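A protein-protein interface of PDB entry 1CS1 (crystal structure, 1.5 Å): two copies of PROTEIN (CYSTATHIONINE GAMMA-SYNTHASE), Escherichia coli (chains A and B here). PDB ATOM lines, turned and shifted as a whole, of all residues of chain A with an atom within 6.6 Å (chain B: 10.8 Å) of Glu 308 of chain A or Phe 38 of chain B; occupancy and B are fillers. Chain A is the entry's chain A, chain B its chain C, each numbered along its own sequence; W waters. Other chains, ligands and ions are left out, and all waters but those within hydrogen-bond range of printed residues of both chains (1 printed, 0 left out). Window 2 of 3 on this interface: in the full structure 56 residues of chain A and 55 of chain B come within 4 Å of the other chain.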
ATOM      1  N   GLY A 306      12.312   5.333   4.309  1.00  0.00           N
ATOM      2  CA  GLY A 306      13.038   4.369   3.502  1.00  0.00           C
ATOM      3  C   GLY A 306      14.444   4.153   4.034  1.00  0.00           C
ATOM      4  O   GLY A 306      14.708   4.330   5.226  1.00  0.00           O
ATOM      5  N   ASP A 307      15.355   3.777   3.148  1.00  0.00           N
ATOM      6  CA  ASP A 307      16.728   3.536   3.545  1.00  0.00           C
ATOM      7  C   ASP A 307      17.717   4.448   2.817  1.00  0.00           C
ATOM      8  O   ASP A 307      17.330   5.444   2.209  1.00  0.00           O
ATOM      9  CB  ASP A 307      17.082   2.060   3.312  1.00  0.00           C
ATOM     10  CG  ASP A 307      17.143   1.685   1.829  1.00  0.00           C
ATOM     11  OD1 ASP A 307      16.831   2.527   0.961  1.00  0.00           O
ATOM     12  OD2 ASP A 307      17.512   0.528   1.532  1.00  0.00           O
ATOM     13  N   GLU A 308      18.998   4.102   2.885  1.00  0.00           N
ATOM     14  CA  GLU A 308      20.025   4.900   2.244  1.00  0.00           C
ATOM     15  C   GLU A 308      19.871   4.974   0.739  1.00  0.00           C
ATOM     16  O   GLU A 308      20.216   5.981   0.126  1.00  0.00           O
ATOM     17  CB  GLU A 308      21.418   4.366   2.572  1.00  0.00           C
ATOM     18  CG  GLU A 308      22.505   5.309   2.119  1.00  0.00           C
ATOM     19  CD  GLU A 308      23.873   4.683   2.154  1.00  0.00           C
ATOM     20  OE1 GLU A 308      24.467   4.606   3.251  1.00  0.00           O
ATOM     21  OE2 GLU A 308      24.357   4.268   1.083  1.00  0.00           O
ATOM     22  N   GLN A 309      19.376   3.908   0.130  1.00  0.00           N
ATOM     23  CA  GLN A 309      19.196   3.935  -1.310  1.00  0.00           C
ATOM     24  C   GLN A 309      17.948   4.745  -1.673  1.00  0.00           C
ATOM     25  O   GLN A 309      17.886   5.356  -2.732  1.00  0.00           O
ATOM     26  CB  GLN A 309      19.114   2.509  -1.854  1.00  0.00           C
ATOM     27  CG  GLN A 309      20.376   1.689  -1.582  1.00  0.00           C
ATOM     28  CD  GLN A 309      21.605   2.216  -2.323  1.00  0.00           C
ATOM     29  OE1 GLN A 309      21.544   2.538  -3.516  1.00  0.00           O
ATOM     30  NE2 GLN A 309      22.731   2.298  -1.614  1.00  0.00           N
ATOM     31  N   THR A 310      16.956   4.754  -0.792  1.00  0.00           N
ATOM     32  CA  THR A 310      15.741   5.525  -1.034  1.00  0.00           C
ATOM     33  C   THR A 310      16.170   6.992  -0.982  1.00  0.00           C
ATOM     34  O   THR A 310      15.730   7.819  -1.778  1.00  0.00           O
ATOM     35  CB  THR A 310      14.678   5.237   0.060  1.00  0.00           C
ATOM     36  OG1 THR A 310      14.346   3.841   0.043  1.00  0.00           O
ATOM     37  CG2 THR A 310      13.404   6.044  -0.179  1.00  0.00           C
ATOM     38  N   LEU A 311      17.065   7.292  -0.048  1.00  0.00           N
ATOM     39  CA  LEU A 311      17.589   8.641   0.125  1.00  0.00           C
ATOM     40  C   LEU A 311      18.451   9.060  -1.077  1.00  0.00           C
ATOM     41  O   LEU A 311      18.314  10.177  -1.580  1.00  0.00           O
ATOM     42  CB  LEU A 311      18.415   8.711   1.412  1.00  0.00           C
ATOM     43  CG  LEU A 311      18.753  10.117   1.908  1.00  0.00           C
ATOM     44  CD1 LEU A 311      18.434  10.265   3.392  1.00  0.00           C
ATOM     45  CD2 LEU A 311      20.222  10.375   1.633  1.00  0.00           C
ATOM     46  N   ARG A 312      19.340   8.166  -1.525  1.00  0.00           N
ATOM     47  CA  ARG A 312      20.206   8.434  -2.674  1.00  0.00           C
ATOM     48  C   ARG A 312      19.344   8.651  -3.912  1.00  0.00           C
ATOM     49  O   ARG A 312      19.688   9.450  -4.786  1.00  0.00           O
ATOM     50  CB  ARG A 312      21.133   7.255  -2.941  1.00  0.00           C
ATOM     51  CG  ARG A 312      22.254   7.103  -1.961  1.00  0.00           C
ATOM     52  CD  ARG A 312      22.927   5.758  -2.169  1.00  0.00           C
ATOM     53  NE  ARG A 312      24.259   5.690  -1.566  1.00  0.00           N
ATOM     54  CZ  ARG A 312      25.269   6.492  -1.891  1.00  0.00           C
ATOM     55  NH1 ARG A 312      25.103   7.431  -2.815  1.00  0.00           N
ATOM     56  NH2 ARG A 312      26.443   6.363  -1.281  1.00  0.00           N
ATOM     57  N   ARG A 313      18.232   7.915  -3.978  1.00  0.00           N
ATOM     58  CA  ARG A 313      17.287   7.994  -5.095  1.00  0.00           C
ATOM     59  C   ARG A 313      16.579   9.339  -5.053  1.00  0.00           C
ATOM     60  O   ARG A 313      16.384   9.994  -6.081  1.00  0.00           O
ATOM     61  CB  ARG A 313      16.234   6.879  -4.993  1.00  0.00           C
ATOM     62  CG  ARG A 313      16.615   5.553  -5.660  1.00  0.00           C
ATOM     63  CD  ARG A 313      15.377   4.752  -6.124  1.00  0.00           C
ATOM     64  NE  ARG A 313      14.464   4.417  -5.029  1.00  0.00           N
ATOM     65  CZ  ARG A 313      14.755   3.583  -4.029  1.00  0.00           C
ATOM     66  NH1 ARG A 313      15.940   2.985  -3.972  1.00  0.00           N
ATOM     67  NH2 ARG A 313      13.862   3.352  -3.077  1.00  0.00           N
ATOM     68  N   LEU A 315      17.617  12.169  -3.562  1.00  0.00           N
ATOM     69  CA  LEU A 315      18.592  13.182  -3.918  1.00  0.00           C
ATOM     70  C   LEU A 315      18.870  13.196  -5.428  1.00  0.00           C
ATOM     71  O   LEU A 315      18.793  14.246  -6.065  1.00  0.00           O
ATOM     72  CB  LEU A 315      19.886  12.958  -3.132  1.00  0.00           C
ATOM     73  CG  LEU A 315      19.766  13.268  -1.633  1.00  0.00           C
ATOM     74  CD1 LEU A 315      21.029  12.830  -0.898  1.00  0.00           C
ATOM     75  CD2 LEU A 315      19.507  14.763  -1.439  1.00  0.00           C
ATOM     76  N   LEU A 323      23.463  20.049  -3.112  1.00  0.00           N
ATOM     77  CA  LEU A 323      23.919  19.244  -1.990  1.00  0.00           C
ATOM     78  C   LEU A 323      25.185  19.906  -1.500  1.00  0.00           C
ATOM     79  O   LEU A 323      26.244  19.796  -2.125  1.00  0.00           O
ATOM     80  CB  LEU A 323      24.238  17.817  -2.437  1.00  0.00           C
ATOM     81  CG  LEU A 323      24.603  16.841  -1.313  1.00  0.00           C
ATOM     82  CD1 LEU A 323      23.397  16.649  -0.418  1.00  0.00           C
ATOM     83  CD2 LEU A 323      25.065  15.502  -1.902  1.00  0.00           C
ATOM     84  N   HIS A 336      22.421  16.279   4.239  1.00  0.00           N
ATOM     85  CA  HIS A 336      22.072  15.053   4.930  1.00  0.00           C
ATOM     86  C   HIS A 336      22.807  15.151   6.249  1.00  0.00           C
ATOM     87  O   HIS A 336      24.030  15.050   6.269  1.00  0.00           O
ATOM     88  CB  HIS A 336      22.599  13.863   4.137  1.00  0.00           C
ATOM     89  CG  HIS A 336      22.307  12.544   4.773  1.00  0.00           C
ATOM     90  ND1 HIS A 336      23.277  11.592   4.996  1.00  0.00           N
ATOM     91  CD2 HIS A 336      21.147  12.015   5.231  1.00  0.00           C
ATOM     92  CE1 HIS A 336      22.729  10.531   5.563  1.00  0.00           C
ATOM     93  NE2 HIS A 336      21.438  10.762   5.718  1.00  0.00           N
ATOM     94  N   THR A 339      25.636  12.575   7.354  1.00  0.00           N
ATOM     95  CA  THR A 339      26.905  12.554   6.641  1.00  0.00           C
ATOM     96  C   THR A 339      27.482  13.943   6.385  1.00  0.00           C
ATOM     97  O   THR A 339      28.549  14.071   5.790  1.00  0.00           O
ATOM     98  CB  THR A 339      26.788  11.816   5.282  1.00  0.00           C
ATOM     99  OG1 THR A 339      25.851  12.492   4.438  1.00  0.00           O
ATOM    100  CG2 THR A 339      26.321  10.399   5.487  1.00  0.00           C
ATOM    101  N   MET A 340      26.803  14.989   6.841  1.00  0.00           N
ATOM    102  CA  MET A 340      27.315  16.327   6.596  1.00  0.00           C
ATOM    103  C   MET A 340      27.452  17.181   7.847  1.00  0.00           C
ATOM    104  O   MET A 340      28.550  17.317   8.396  1.00  0.00           O
ATOM    105  CB  MET A 340      26.442  17.007   5.539  1.00  0.00           C
ATOM    106  CG  MET A 340      26.535  16.251   4.222  1.00  0.00           C
ATOM    107  SD  MET A 340      25.499  16.748   2.835  1.00  0.00           S
ATOM    108  CE  MET A 340      26.020  18.466   2.635  1.00  0.00           C
ATOM    109  N   GLU A 357      18.908   8.819  10.472  1.00  0.00           N
ATOM    110  CA  GLU A 357      19.887   8.578   9.417  1.00  0.00           C
ATOM    111  C   GLU A 357      19.350   8.974   8.047  1.00  0.00           C
ATOM    112  O   GLU A 357      20.085   8.950   7.058  1.00  0.00           O
ATOM    113  CB  GLU A 357      20.286   7.106   9.386  1.00  0.00           C
ATOM    114  CG  GLU A 357      21.063   6.675  10.599  1.00  0.00           C
ATOM    115  CD  GLU A 357      22.389   7.386  10.700  1.00  0.00           C
ATOM    116  OE1 GLU A 357      23.239   7.162   9.814  1.00  0.00           O
ATOM    117  OE2 GLU A 357      22.583   8.165  11.658  1.00  0.00           O
ATOM    118  N   THR A 358      18.067   9.321   7.990  1.00  0.00           N
ATOM    119  CA  THR A 358      17.441   9.736   6.734  1.00  0.00           C
ATOM    120  C   THR A 358      16.891  11.167   6.824  1.00  0.00           C
ATOM    121  O   THR A 358      16.013  11.566   6.052  1.00  0.00           O
ATOM    122  CB  THR A 358      16.302   8.761   6.317  1.00  0.00           C
ATOM    123  OG1 THR A 358      15.293   8.706   7.337  1.00  0.00           O
ATOM    124  CG2 THR A 358      16.866   7.370   6.099  1.00  0.00           C
ATOM    125  N   LEU A 360      16.926  15.032   6.224  1.00  0.00           N
ATOM    126  CA  LEU A 360      17.451  15.972   5.242  1.00  0.00           C
ATOM    127  C   LEU A 360      17.014  17.370   5.687  1.00  0.00           C
ATOM    128  O   LEU A 360      15.857  17.579   6.098  1.00  0.00           O
ATOM    129  CB  LEU A 360      16.890  15.664   3.848  1.00  0.00           C
ATOM    130  CG  LEU A 360      17.385  14.343   3.238  1.00  0.00           C
ATOM    131  CD1 LEU A 360      16.611  14.033   1.971  1.00  0.00           C
ATOM    132  CD2 LEU A 360      18.875  14.439   2.937  1.00  0.00           C
ATOM    133  N   ASN B  34      29.806  22.291  -3.543  1.00  0.00           N
ATOM    134  CA  ASN B  34      28.898  21.159  -3.708  1.00  0.00           C
ATOM    135  C   ASN B  34      29.636  19.825  -3.637  1.00  0.00           C
ATOM    136  O   ASN B  34      30.840  19.740  -3.905  1.00  0.00           O
ATOM    137  CB  ASN B  34      28.159  21.258  -5.054  1.00  0.00           C
ATOM    138  CG  ASN B  34      29.068  20.988  -6.253  1.00  0.00           C
ATOM    139  OD1 ASN B  34      29.601  19.889  -6.414  1.00  0.00           O
ATOM    140  ND2 ASN B  34      29.243  21.998  -7.102  1.00  0.00           N
ATOM    141  N   PHE B  35      28.907  18.782  -3.258  1.00  0.00           N
ATOM    142  CA  PHE B  35      29.477  17.439  -3.196  1.00  0.00           C
ATOM    143  C   PHE B  35      29.317  16.869  -4.601  1.00  0.00           C
ATOM    144  O   PHE B  35      28.479  17.340  -5.376  1.00  0.00           O
ATOM    145  CB  PHE B  35      28.683  16.552  -2.230  1.00  0.00           C
ATOM    146  CG  PHE B  35      29.028  16.745  -0.784  1.00  0.00           C
ATOM    147  CD1 PHE B  35      29.397  18.003  -0.293  1.00  0.00           C
ATOM    148  CD2 PHE B  35      28.937  15.668   0.104  1.00  0.00           C
ATOM    149  CE1 PHE B  35      29.660  18.190   1.055  1.00  0.00           C
ATOM    150  CE2 PHE B  35      29.199  15.838   1.461  1.00  0.00           C
ATOM    151  CZ  PHE B  35      29.562  17.104   1.941  1.00  0.00           C
ATOM    152  N   THR B  36      30.106  15.854  -4.937  1.00  0.00           N
ATOM    153  CA  THR B  36      29.975  15.236  -6.254  1.00  0.00           C
ATOM    154  C   THR B  36      28.812  14.233  -6.179  1.00  0.00           C
ATOM    155  O   THR B  36      28.139  13.941  -7.176  1.00  0.00           O
ATOM    156  CB  THR B  36      31.268  14.520  -6.649  1.00  0.00           C
ATOM    157  OG1 THR B  36      31.916  14.032  -5.468  1.00  0.00           O
ATOM    158  CG2 THR B  36      32.201  15.483  -7.372  1.00  0.00           C
ATOM    159  N   GLY B  37      28.576  13.730  -4.972  1.00  0.00           N
ATOM    160  CA  GLY B  37      27.499  12.782  -4.741  1.00  0.00           C
ATOM    161  C   GLY B  37      27.218  12.692  -3.255  1.00  0.00           C
ATOM    162  O   GLY B  37      27.938  13.295  -2.457  1.00  0.00           O
ATOM    163  N   PHE B  38      26.177  11.962  -2.873  1.00  0.00           N
ATOM    164  CA  PHE B  38      25.848  11.815  -1.460  1.00  0.00           C
ATOM    165  C   PHE B  38      27.075  11.227  -0.751  1.00  0.00           C
ATOM    166  O   PHE B  38      27.707  10.283  -1.251  1.00  0.00           O
ATOM    167  CB  PHE B  38      24.618  10.896  -1.301  1.00  0.00           C
ATOM    168  CG  PHE B  38      24.472  10.281   0.074  1.00  0.00           C
ATOM    169  CD1 PHE B  38      23.704  10.902   1.046  1.00  0.00           C
ATOM    170  CD2 PHE B  38      25.093   9.066   0.383  1.00  0.00           C
ATOM    171  CE1 PHE B  38      23.557  10.322   2.302  1.00  0.00           C
ATOM    172  CE2 PHE B  38      24.950   8.480   1.639  1.00  0.00           C
ATOM    173  CZ  PHE B  38      24.183   9.107   2.597  1.00  0.00           C
ATOM    174  N   ASN B  39      27.435  11.816   0.386  1.00  0.00           N
ATOM    175  CA  ASN B  39      28.575  11.357   1.177  1.00  0.00           C
ATOM    176  C   ASN B  39      29.899  11.352   0.393  1.00  0.00           C
ATOM    177  O   ASN B  39      30.825  10.615   0.741  1.00  0.00           O
ATOM    178  CB  ASN B  39      28.293   9.954   1.728  1.00  0.00           C
ATOM    179  CG  ASN B  39      29.221   9.572   2.864  1.00  0.00           C
ATOM    180  OD1 ASN B  39      29.517  10.378   3.751  1.00  0.00           O
ATOM    181  ND2 ASN B  39      29.688   8.332   2.843  1.00  0.00           N
ATOM    182  N   GLU B  40      29.980  12.169  -0.658  1.00  0.00           N
ATOM    183  CA  GLU B  40      31.192  12.271  -1.479  1.00  0.00           C
ATOM    184  C   GLU B  40      31.594  13.740  -1.665  1.00  0.00           C
ATOM    185  O   GLU B  40      31.355  14.347  -2.712  1.00  0.00           O
ATOM    186  CB  GLU B  40      30.986  11.585  -2.857  1.00  0.00           C
ATOM    187  N   PRO B  41      32.208  14.331  -0.630  1.00  0.00           N
ATOM    188  CA  PRO B  41      32.625  15.730  -0.734  1.00  0.00           C
ATOM    189  C   PRO B  41      33.870  15.836  -1.581  1.00  0.00           C
ATOM    190  O   PRO B  41      34.532  14.840  -1.863  1.00  0.00           O
ATOM    191  CB  PRO B  41      32.911  16.127   0.714  1.00  0.00           C
ATOM    192  CG  PRO B  41      33.380  14.850   1.342  1.00  0.00           C
ATOM    193  CD  PRO B  41      32.549  13.757   0.686  1.00  0.00           C
ATOM    194  N   ARG B  42      34.184  17.057  -1.986  1.00  0.00           N
ATOM    195  CA  ARG B  42      35.378  17.305  -2.765  1.00  0.00           C
ATOM    196  C   ARG B  42      36.494  17.715  -1.789  1.00  0.00           C
ATOM    197  O   ARG B  42      36.318  17.661  -0.565  1.00  0.00           O
ATOM    198  CB  ARG B  42      35.116  18.427  -3.766  1.00  0.00           C
ATOM    199  CG  ARG B  42      33.901  18.226  -4.651  1.00  0.00           C
ATOM    200  CD  ARG B  42      33.674  19.505  -5.442  1.00  0.00           C
ATOM    201  NE  ARG B  42      32.561  19.438  -6.384  1.00  0.00           N
ATOM    202  CZ  ARG B  42      32.716  19.361  -7.700  1.00  0.00           C
ATOM    203  NH1 ARG B  42      33.937  19.339  -8.219  1.00  0.00           N
ATOM    204  NH2 ARG B  42      31.658  19.328  -8.497  1.00  0.00           N
HETATM  205  O   HOH W   1      25.977  13.182   1.782  1.00  0.00           O
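The backbone carbonyl oxygen of Leu 323 of chain A lies within hydrogen-bond range of the backbone NH of Phe 35 of chain B, 3.1 Å away.
Of the 16 printed residues of chain A, 8 touch a printed residue of chain B. Printed residues of chain A that touch a printed residue of chain B: Glu 308, Leu 311, Arg 312, Leu 315, Leu 323, His 336, Thr 339 and Met 340. Among the printed residues, 12 pairs touch across the chains. Among the printed residues, no Asp or Glu carboxylate lies within 4 Å of a Lys or Arg side-chain nitrogen of the other chain.
The backbone carbonyl oxygen of Glu 357 of chain A sits at hydrogen-bond distance from a ring nitrogen (NE2) of His 336 of chain A (2.6 Å). NE of Arg 312 of chain A is in salt-bridge range of OE2 of Glu 308 of chain A, at 3.0 Å. The side-chain amide oxygen of Asn 34 of chain B sits at hydrogen-bond distance from the guanidinium group of Arg 42 of chain B (3.0 Å). ND1 of His 336 of chain A sits at hydrogen-bond distance from OG1 of Thr 339 of chain A, at 2.8 Å. The backbone NH (N) of His 336 of chain A sits at hydrogen-bond distance from the side-chain sulfur (SD) of Met 340 of chain A.
Of the printed residues of chain B, Glu 308 of chain A touches Phe 38 (3.98 Å). Of the printed residues of chain A, Phe 38 of chain B touches Glu 308, Leu 311, Arg 312, Leu 315, Leu 323, His 336 and Thr 339. Asp 307 of chain A touches none of the printed residues of chain B. Gln 309 of chain A touches none of the printed residues of chain B. No residue of chain B comes within 4 Å of Thr 310 of chain A. Of the printed residues of chain B, Leu 311 of chain A touches Phe 38 (3.4 Å). Of the printed residues of chain B, His 336 of chain A touches Phe 38. Of the printed residues of chain B, Thr 339 of chain A touches Phe 38 and Asn 39. Of the printed residues of chain B, Leu 323 of chain A touches Asn 34, Phe 35, Gly 37 and Phe 38. Of the printed residues of chain A, Asn 39 of chain B touches Thr 339. Printed residues of chain B within 4 Å of Leu 315 of chain A: Phe 38 (3.8 Å). Printed residues of chain A within 4 Å of Asn 34 of chain B: Leu 323. The nearest printed residue of chain B that does not touch Glu 308 of chain A is Asn 39 of chain B (6.4 Å). The nearest printed residue of chain A that does not touch Asn 39 of chain B is Leu 323 of chain A (4.9 Å).
Water W1 lies within hydrogen-bond range of the backbone NH of Asn 39 of chain B (2.4 Å), the side-chain hydroxyl of Thr 339 of chain A (2.7 Å) and the side-chain sulfur of Met 340 of chain A (3.7 Å).
No position is printed for both chains.
Among the printed residues, merely in contact across the chains: Glu 308 of chain A with Phe 38 of chain B, Leu 311 of chain A with Phe 38 of chain B, Arg 312 of chain A with Phe 38 of chain B, Leu 315 of chain A with Phe 38 of chain B, Leu 323 of chain A with Asn 34 of chain B, Leu 323 of chain A with Gly 37 of chain B, Leu 323 of chain A with Phe 38 of chain B, His 336 of chain A with Phe 38 of chain B, Thr 339 of chain A with Phe 38 of chain B, Thr 339 of chain A with Asn 39 of chain B and Met 340 of chain A with Phe 35 of chain B.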
